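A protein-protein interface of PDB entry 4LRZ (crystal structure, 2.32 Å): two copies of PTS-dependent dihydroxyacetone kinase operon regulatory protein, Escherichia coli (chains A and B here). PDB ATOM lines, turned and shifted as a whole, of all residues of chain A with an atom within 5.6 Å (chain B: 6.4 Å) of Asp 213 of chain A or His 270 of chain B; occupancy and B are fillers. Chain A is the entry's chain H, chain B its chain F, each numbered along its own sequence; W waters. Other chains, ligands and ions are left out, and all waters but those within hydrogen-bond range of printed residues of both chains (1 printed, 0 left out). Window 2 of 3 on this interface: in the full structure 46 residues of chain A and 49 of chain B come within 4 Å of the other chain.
N of Asp 213 of chain A sits at hydrogen-bond distance from OD2 of Asp 214 of chain B (2.8 Å).
OD2 of Asp 213 of chain A is in hydrogen-bond range of ND1 of His 304 of chain B, at 2.7 Å.
The backbone NH (N) of Asp 213 of chain B lies within hydrogen-bond range of the side-chain carboxylate (OD2) of Asp 214 of chain A, at 3.2 Å.
The backbone carbonyl oxygen of Thr 287 of chain B lies within hydrogen-bond range of the backbone NH of Leu 302 of chain B, 3.0 Å away.
The backbone NH (N) of His 304 of chain B lies within hydrogen-bond range of the backbone carbonyl oxygen (O) of Val 285 of chain B (2.8 Å).
The backbone carbonyl oxygen of Ile 286 of chain B lies within hydrogen-bond range of the backbone NH of His 270 of chain B (3.0 Å).
The side-chain hydroxyl (OG1) of Thr 287 of chain B is in hydrogen-bond range of the backbone NH (N) of His 270 of chain B, at 3.2 Å.
The backbone carbonyl oxygen (O) of Met 212 of chain A sits at hydrogen-bond distance from the side-chain amide nitrogen (NE2) of Gln 231 of chain A.
The side-chain carboxylate (OD1) of Asp 214 of chain B sits at hydrogen-bond distance from a ring nitrogen (ND1) of His 304 of chain B.
Among the printed residues, merely in contact across the chains: Asp 213 of chain A with His 270 of chain B (3.1 Å), Ser 211 of chain A with Leu 302 of chain B (3.5 Å), Met 212 of chain A with Asp 214 of chain B (3.6 Å) and Met 212 of chain A with Leu 302 of chain B (3.8 Å).
Printed residues of chain B within 4 Å of Met 212 of chain A: Asp 214 and Leu 302.
Of chain B, only Asp 214 (2.8 Å), His 270 (3.1 Å) and His 304 (2.7 Å) come within 4 Å of Asp 213 of chain A.
Of the printed residues of chain A, Asp 214 of chain B touches Met 212 (3.6 Å) and Asp 213 (2.8 Å).
His 270 of chain B touches one residue of chain A.
Printed residues of chain A within 4 Å of Leu 302 of chain B: Ser 211 (3.5 Å) and Met 212 (3.8 Å).
The nearest printed residue of chain A that does not touch His 270 of chain B is Ser 211 of chain A (5.9 Å).
The nearest printed residue of chain B that does not touch Ser 211 of chain A is Thr 287 of chain B (4.3 Å).
Hydrophobic or aromatic side chains of chain B within 4 Å of the printed part of chain A: His 270, Leu 302 and His 304.
Along chain B the printed residues that touch a printed residue of chain A span positions 213 to 304.
Asp 213 of chain A touches Asp 214 of chain B, and with the chains exchanged Asp 214 of chain A touches Asp 213 of chain B.
Positions printed for both chains: 213, 214 and 305.
Water W1 lies within hydrogen-bond range of OD2 of Asp 214 of chain B and N of Asp 214 of chain A.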
ATOM      1  N   SER A 211      10.970  25.869  -0.037  1.00  0.00           N
ATOM      2  CA  SER A 211      11.073  24.459  -0.359  1.00  0.00           C
ATOM      3  C   SER A 211      11.739  23.630   0.742  1.00  0.00           C
ATOM      4  O   SER A 211      11.511  22.436   0.855  1.00  0.00           O
ATOM      5  CB  SER A 211      11.818  24.295  -1.675  1.00  0.00           C
ATOM      6  OG  SER A 211      13.063  24.984  -1.621  1.00  0.00           O
ATOM      7  N   MET A 212      12.556  24.252   1.569  1.00  0.00           N
ATOM      8  CA  MET A 212      13.279  23.492   2.588  1.00  0.00           C
ATOM      9  C   MET A 212      12.350  22.964   3.666  1.00  0.00           C
ATOM     10  O   MET A 212      11.243  23.471   3.830  1.00  0.00           O
ATOM     11  CB  MET A 212      14.315  24.364   3.237  1.00  0.00           C
ATOM     12  CG  MET A 212      13.729  25.447   4.065  1.00  0.00           C
ATOM     13  SD  MET A 212      15.028  26.644   4.242  1.00  0.00           S
ATOM     14  CE  MET A 212      14.160  27.936   5.059  1.00  0.00           C
ATOM     15  N   ASP A 213      12.827  21.972   4.422  1.00  0.00           N
ATOM     16  CA  ASP A 213      12.032  21.326   5.454  1.00  0.00           C
ATOM     17  C   ASP A 213      11.955  22.133   6.738  1.00  0.00           C
ATOM     18  O   ASP A 213      10.912  22.180   7.367  1.00  0.00           O
ATOM     19  CB  ASP A 213      12.560  19.914   5.729  1.00  0.00           C
ATOM     20  CG  ASP A 213      12.229  18.921   4.598  1.00  0.00           C
ATOM     21  OD1 ASP A 213      11.287  19.164   3.794  1.00  0.00           O
ATOM     22  OD2 ASP A 213      12.919  17.887   4.520  1.00  0.00           O
ATOM     23  N   ASP A 214      13.044  22.790   7.113  1.00  0.00           N
ATOM     24  CA  ASP A 214      13.073  23.560   8.350  1.00  0.00           C
ATOM     25  C   ASP A 214      12.140  24.763   8.383  1.00  0.00           C
ATOM     26  O   ASP A 214      11.858  25.402   7.363  1.00  0.00           O
ATOM     27  CB  ASP A 214      14.495  23.997   8.660  1.00  0.00           C
ATOM     28  CG  ASP A 214      15.362  22.835   9.214  1.00  0.00           C
ATOM     29  OD1 ASP A 214      14.800  21.774   9.589  1.00  0.00           O
ATOM     30  OD2 ASP A 214      16.602  22.993   9.301  1.00  0.00           O
ATOM     31  N   GLY A 215      11.644  25.075   9.565  1.00  0.00           N
ATOM     32  CA  GLY A 215      10.989  26.357   9.756  1.00  0.00           C
ATOM     33  C   GLY A 215      12.038  27.434   9.902  1.00  0.00           C
ATOM     34  O   GLY A 215      13.126  27.193  10.451  1.00  0.00           O
ATOM     35  N   GLN A 231       6.394  27.167   6.997  1.00  0.00           N
ATOM     36  CA  GLN A 231       6.640  26.132   7.985  1.00  0.00           C
ATOM     37  C   GLN A 231       6.722  26.747   9.396  1.00  0.00           C
ATOM     38  O   GLN A 231       6.004  26.319  10.296  1.00  0.00           O
ATOM     39  CB  GLN A 231       7.907  25.315   7.595  1.00  0.00           C
ATOM     40  CG  GLN A 231       7.883  24.643   6.142  1.00  0.00           C
ATOM     41  CD  GLN A 231       8.261  25.595   4.938  1.00  0.00           C
ATOM     42  OE1 GLN A 231       7.547  26.571   4.635  1.00  0.00           O
ATOM     43  NE2 GLN A 231       9.369  25.279   4.241  1.00  0.00           N
ATOM     44  N   LEU A 303      13.625  26.006  13.001  1.00  0.00           N
ATOM     45  CA  LEU A 303      12.852  25.102  13.799  1.00  0.00           C
ATOM     46  C   LEU A 303      12.917  23.792  13.075  1.00  0.00           C
ATOM     47  O   LEU A 303      12.285  23.600  12.034  1.00  0.00           O
ATOM     48  CB  LEU A 303      11.418  25.587  13.944  1.00  0.00           C
ATOM     49  CG  LEU A 303      11.200  27.037  14.380  1.00  0.00           C
ATOM     50  CD1 LEU A 303       9.812  27.464  13.949  1.00  0.00           C
ATOM     51  CD2 LEU A 303      11.327  27.257  15.859  1.00  0.00           C
ATOM     52  N   PRO A 305      12.352  19.912  12.253  1.00  0.00           N
ATOM     53  CA  PRO A 305      11.084  19.205  12.338  1.00  0.00           C
ATOM     54  C   PRO A 305      11.270  17.902  13.093  1.00  0.00           C
ATOM     55  O   PRO A 305      11.810  16.940  12.543  1.00  0.00           O
ATOM     56  CB  PRO A 305      10.722  18.957  10.860  1.00  0.00           C
ATOM     57  CG  PRO A 305      11.808  19.670  10.028  1.00  0.00           C
ATOM     58  CD  PRO A 305      12.992  19.710  10.943  1.00  0.00           C
ATOM     59  N   ASP B 213      19.228  21.924   7.782  1.00  0.00           N
ATOM     60  CA  ASP B 213      19.385  20.461   7.770  1.00  0.00           C
ATOM     61  C   ASP B 213      19.504  19.851   6.403  1.00  0.00           C
ATOM     62  O   ASP B 213      20.281  18.935   6.209  1.00  0.00           O
ATOM     63  CB  ASP B 213      18.248  19.765   8.517  1.00  0.00           C
ATOM     64  CG  ASP B 213      18.460  19.737  10.024  1.00  0.00           C
ATOM     65  OD1 ASP B 213      19.606  19.952  10.492  1.00  0.00           O
ATOM     66  OD2 ASP B 213      17.468  19.507  10.745  1.00  0.00           O
ATOM     67  N   ASP B 214      18.755  20.355   5.444  1.00  0.00           N
ATOM     68  CA  ASP B 214      18.770  19.758   4.126  1.00  0.00           C
ATOM     69  C   ASP B 214      20.100  20.022   3.454  1.00  0.00           C
ATOM     70  O   ASP B 214      20.720  21.052   3.697  1.00  0.00           O
ATOM     71  CB  ASP B 214      17.636  20.328   3.272  1.00  0.00           C
ATOM     72  CG  ASP B 214      16.255  19.933   3.792  1.00  0.00           C
ATOM     73  OD1 ASP B 214      16.068  18.730   4.128  1.00  0.00           O
ATOM     74  OD2 ASP B 214      15.375  20.833   3.882  1.00  0.00           O
ATOM     75  N   LEU B 268       9.512  18.726  -8.024  1.00  0.00           N
ATOM     76  CA  LEU B 268       9.467  17.391  -7.428  1.00  0.00           C
ATOM     77  C   LEU B 268       9.563  17.540  -5.927  1.00  0.00           C
ATOM     78  O   LEU B 268      10.462  18.224  -5.442  1.00  0.00           O
ATOM     79  CB  LEU B 268      10.644  16.542  -7.903  1.00  0.00           C
ATOM     80  CG  LEU B 268      10.631  15.982  -9.321  1.00  0.00           C
ATOM     81  CD1 LEU B 268      11.998  15.444  -9.676  1.00  0.00           C
ATOM     82  CD2 LEU B 268       9.568  14.885  -9.466  1.00  0.00           C
ATOM     83  N   LYS B 269       8.653  16.905  -5.189  1.00  0.00           N
ATOM     84  CA  LYS B 269       8.636  17.028  -3.728  1.00  0.00           C
ATOM     85  C   LYS B 269       8.790  15.683  -3.024  1.00  0.00           C
ATOM     86  O   LYS B 269       8.049  14.738  -3.306  1.00  0.00           O
ATOM     87  CB  LYS B 269       7.373  17.758  -3.262  1.00  0.00           C
ATOM     88  CG  LYS B 269       6.982  18.922  -4.176  1.00  0.00           C
ATOM     89  CD  LYS B 269       6.122  19.989  -3.507  1.00  0.00           C
ATOM     90  CE  LYS B 269       5.915  21.161  -4.468  1.00  0.00           C
ATOM     91  NZ  LYS B 269       5.157  22.289  -3.861  1.00  0.00           N
ATOM     92  N   HIS B 270       9.773  15.598  -2.125  1.00  0.00           N
ATOM     93  CA  HIS B 270      10.037  14.397  -1.308  1.00  0.00           C
ATOM     94  C   HIS B 270      10.056  13.078  -2.101  1.00  0.00           C
ATOM     95  O   HIS B 270       9.676  12.034  -1.582  1.00  0.00           O
ATOM     96  CB  HIS B 270       9.038  14.300  -0.136  1.00  0.00           C
ATOM     97  CG  HIS B 270       9.399  15.140   1.056  1.00  0.00           C
ATOM     98  ND1 HIS B 270       9.474  16.519   1.010  1.00  0.00           N
ATOM     99  CD2 HIS B 270       9.671  14.794   2.340  1.00  0.00           C
ATOM    100  CE1 HIS B 270       9.797  16.983   2.206  1.00  0.00           C
ATOM    101  NE2 HIS B 270       9.920  15.958   3.032  1.00  0.00           N
ATOM    102  N   VAL B 271      10.506  13.140  -3.352  1.00  0.00           N
ATOM    103  CA  VAL B 271      10.597  11.975  -4.245  1.00  0.00           C
ATOM    104  C   VAL B 271      11.900  11.172  -4.010  1.00  0.00           C
ATOM    105  O   VAL B 271      12.910  11.746  -3.590  1.00  0.00           O
ATOM    106  CB  VAL B 271      10.520  12.437  -5.734  1.00  0.00           C
ATOM    107  CG1 VAL B 271      10.549  11.251  -6.695  1.00  0.00           C
ATOM    108  CG2 VAL B 271       9.274  13.284  -5.979  1.00  0.00           C
ATOM    109  N   GLU B 272      11.882   9.861  -4.288  1.00  0.00           N
ATOM    110  CA  GLU B 272      13.103   9.030  -4.244  1.00  0.00           C
ATOM    111  C   GLU B 272      13.994   9.216  -5.477  1.00  0.00           C
ATOM    112  O   GLU B 272      13.493   9.433  -6.586  1.00  0.00           O
ATOM    113  CB  GLU B 272      12.768   7.544  -4.110  1.00  0.00           C
ATOM    114  CG  GLU B 272      12.089   7.132  -2.810  1.00  0.00           C
ATOM    115  CD  GLU B 272      11.922   5.620  -2.707  1.00  0.00           C
ATOM    116  OE1 GLU B 272      12.934   4.915  -2.500  1.00  0.00           O
ATOM    117  OE2 GLU B 272      10.781   5.135  -2.839  1.00  0.00           O
ATOM    118  N   VAL B 285      16.322  11.060  -0.847  1.00  0.00           N
ATOM    119  CA  VAL B 285      15.011  11.655  -1.050  1.00  0.00           C
ATOM    120  C   VAL B 285      15.211  13.150  -1.336  1.00  0.00           C
ATOM    121  O   VAL B 285      15.903  13.852  -0.598  1.00  0.00           O
ATOM    122  CB  VAL B 285      14.045  11.376   0.138  1.00  0.00           C
ATOM    123  CG1 VAL B 285      14.780  11.451   1.476  1.00  0.00           C
ATOM    124  CG2 VAL B 285      12.836  12.316   0.118  1.00  0.00           C
ATOM    125  N   ILE B 286      14.626  13.616  -2.429  1.00  0.00           N
ATOM    126  CA  ILE B 286      14.950  14.928  -2.938  1.00  0.00           C
ATOM    127  C   ILE B 286      13.724  15.800  -3.091  1.00  0.00           C
ATOM    128  O   ILE B 286      12.606  15.306  -3.059  1.00  0.00           O
ATOM    129  CB  ILE B 286      15.652  14.825  -4.299  1.00  0.00           C
ATOM    130  CG1 ILE B 286      14.653  14.410  -5.376  1.00  0.00           C
ATOM    131  CG2 ILE B 286      16.819  13.859  -4.223  1.00  0.00           C
ATOM    132  CD1 ILE B 286      14.985  14.885  -6.747  1.00  0.00           C
ATOM    133  N   THR B 287      13.960  17.102  -3.254  1.00  0.00           N
ATOM    134  CA  THR B 287      12.972  18.069  -3.751  1.00  0.00           C
ATOM    135  C   THR B 287      13.649  18.879  -4.836  1.00  0.00           C
ATOM    136  O   THR B 287      14.826  19.207  -4.725  1.00  0.00           O
ATOM    137  CB  THR B 287      12.442  19.006  -2.628  1.00  0.00           C
ATOM    138  OG1 THR B 287      11.440  18.322  -1.863  1.00  0.00           O
ATOM    139  CG2 THR B 287      11.815  20.276  -3.196  1.00  0.00           C
ATOM    140  N   LEU B 288      12.925  19.171  -5.904  1.00  0.00           N
ATOM    141  CA  LEU B 288      13.458  20.026  -6.951  1.00  0.00           C
ATOM    142  C   LEU B 288      12.612  21.253  -7.076  1.00  0.00           C
ATOM    143  O   LEU B 288      11.435  21.162  -7.360  1.00  0.00           O
ATOM    144  CB  LEU B 288      13.533  19.329  -8.312  1.00  0.00           C
ATOM    145  CG  LEU B 288      14.133  20.276  -9.365  1.00  0.00           C
ATOM    146  CD1 LEU B 288      15.645  20.165  -9.384  1.00  0.00           C
ATOM    147  CD2 LEU B 288      13.576  20.009 -10.750  1.00  0.00           C
ATOM    148  N   LEU B 302      17.220  19.957  -3.146  1.00  0.00           N
ATOM    149  CA  LEU B 302      17.421  19.638  -1.747  1.00  0.00           C
ATOM    150  C   LEU B 302      17.491  18.146  -1.485  1.00  0.00           C
ATOM    151  O   LEU B 302      16.697  17.358  -2.006  1.00  0.00           O
ATOM    152  CB  LEU B 302      16.342  20.262  -0.873  1.00  0.00           C
ATOM    153  CG  LEU B 302      16.320  21.774  -0.963  1.00  0.00           C
ATOM    154  CD1 LEU B 302      15.185  22.211  -1.834  1.00  0.00           C
ATOM    155  CD2 LEU B 302      16.110  22.311   0.385  1.00  0.00           C
ATOM    156  N   HIS B 304      17.097  15.591   1.283  1.00  0.00           N
ATOM    157  CA  HIS B 304      16.455  15.461   2.575  1.00  0.00           C
ATOM    158  C   HIS B 304      17.145  14.334   3.341  1.00  0.00           C
ATOM    159  O   HIS B 304      17.426  13.282   2.781  1.00  0.00           O
ATOM    160  CB  HIS B 304      14.943  15.207   2.404  1.00  0.00           C
ATOM    161  CG  HIS B 304      14.237  16.251   1.581  1.00  0.00           C
ATOM    162  ND1 HIS B 304      13.955  17.519   2.054  1.00  0.00           N
ATOM    163  CD2 HIS B 304      13.737  16.206   0.323  1.00  0.00           C
ATOM    164  CE1 HIS B 304      13.319  18.209   1.124  1.00  0.00           C
ATOM    165  NE2 HIS B 304      13.177  17.436   0.062  1.00  0.00           N
ATOM    166  N   PRO B 305      17.469  14.576   4.615  1.00  0.00           N
ATOM    167  CA  PRO B 305      18.103  13.505   5.389  1.00  0.00           C
ATOM    168  C   PRO B 305      17.056  12.452   5.796  1.00  0.00           C
ATOM    169  O   PRO B 305      15.936  12.825   6.153  1.00  0.00           O
ATOM    170  CB  PRO B 305      18.682  14.247   6.605  1.00  0.00           C
ATOM    171  CG  PRO B 305      17.852  15.516   6.725  1.00  0.00           C
ATOM    172  CD  PRO B 305      17.342  15.845   5.363  1.00  0.00           C
HETATM  173  O   HOH W   1      15.954  22.474   5.982  1.00  0.00           O
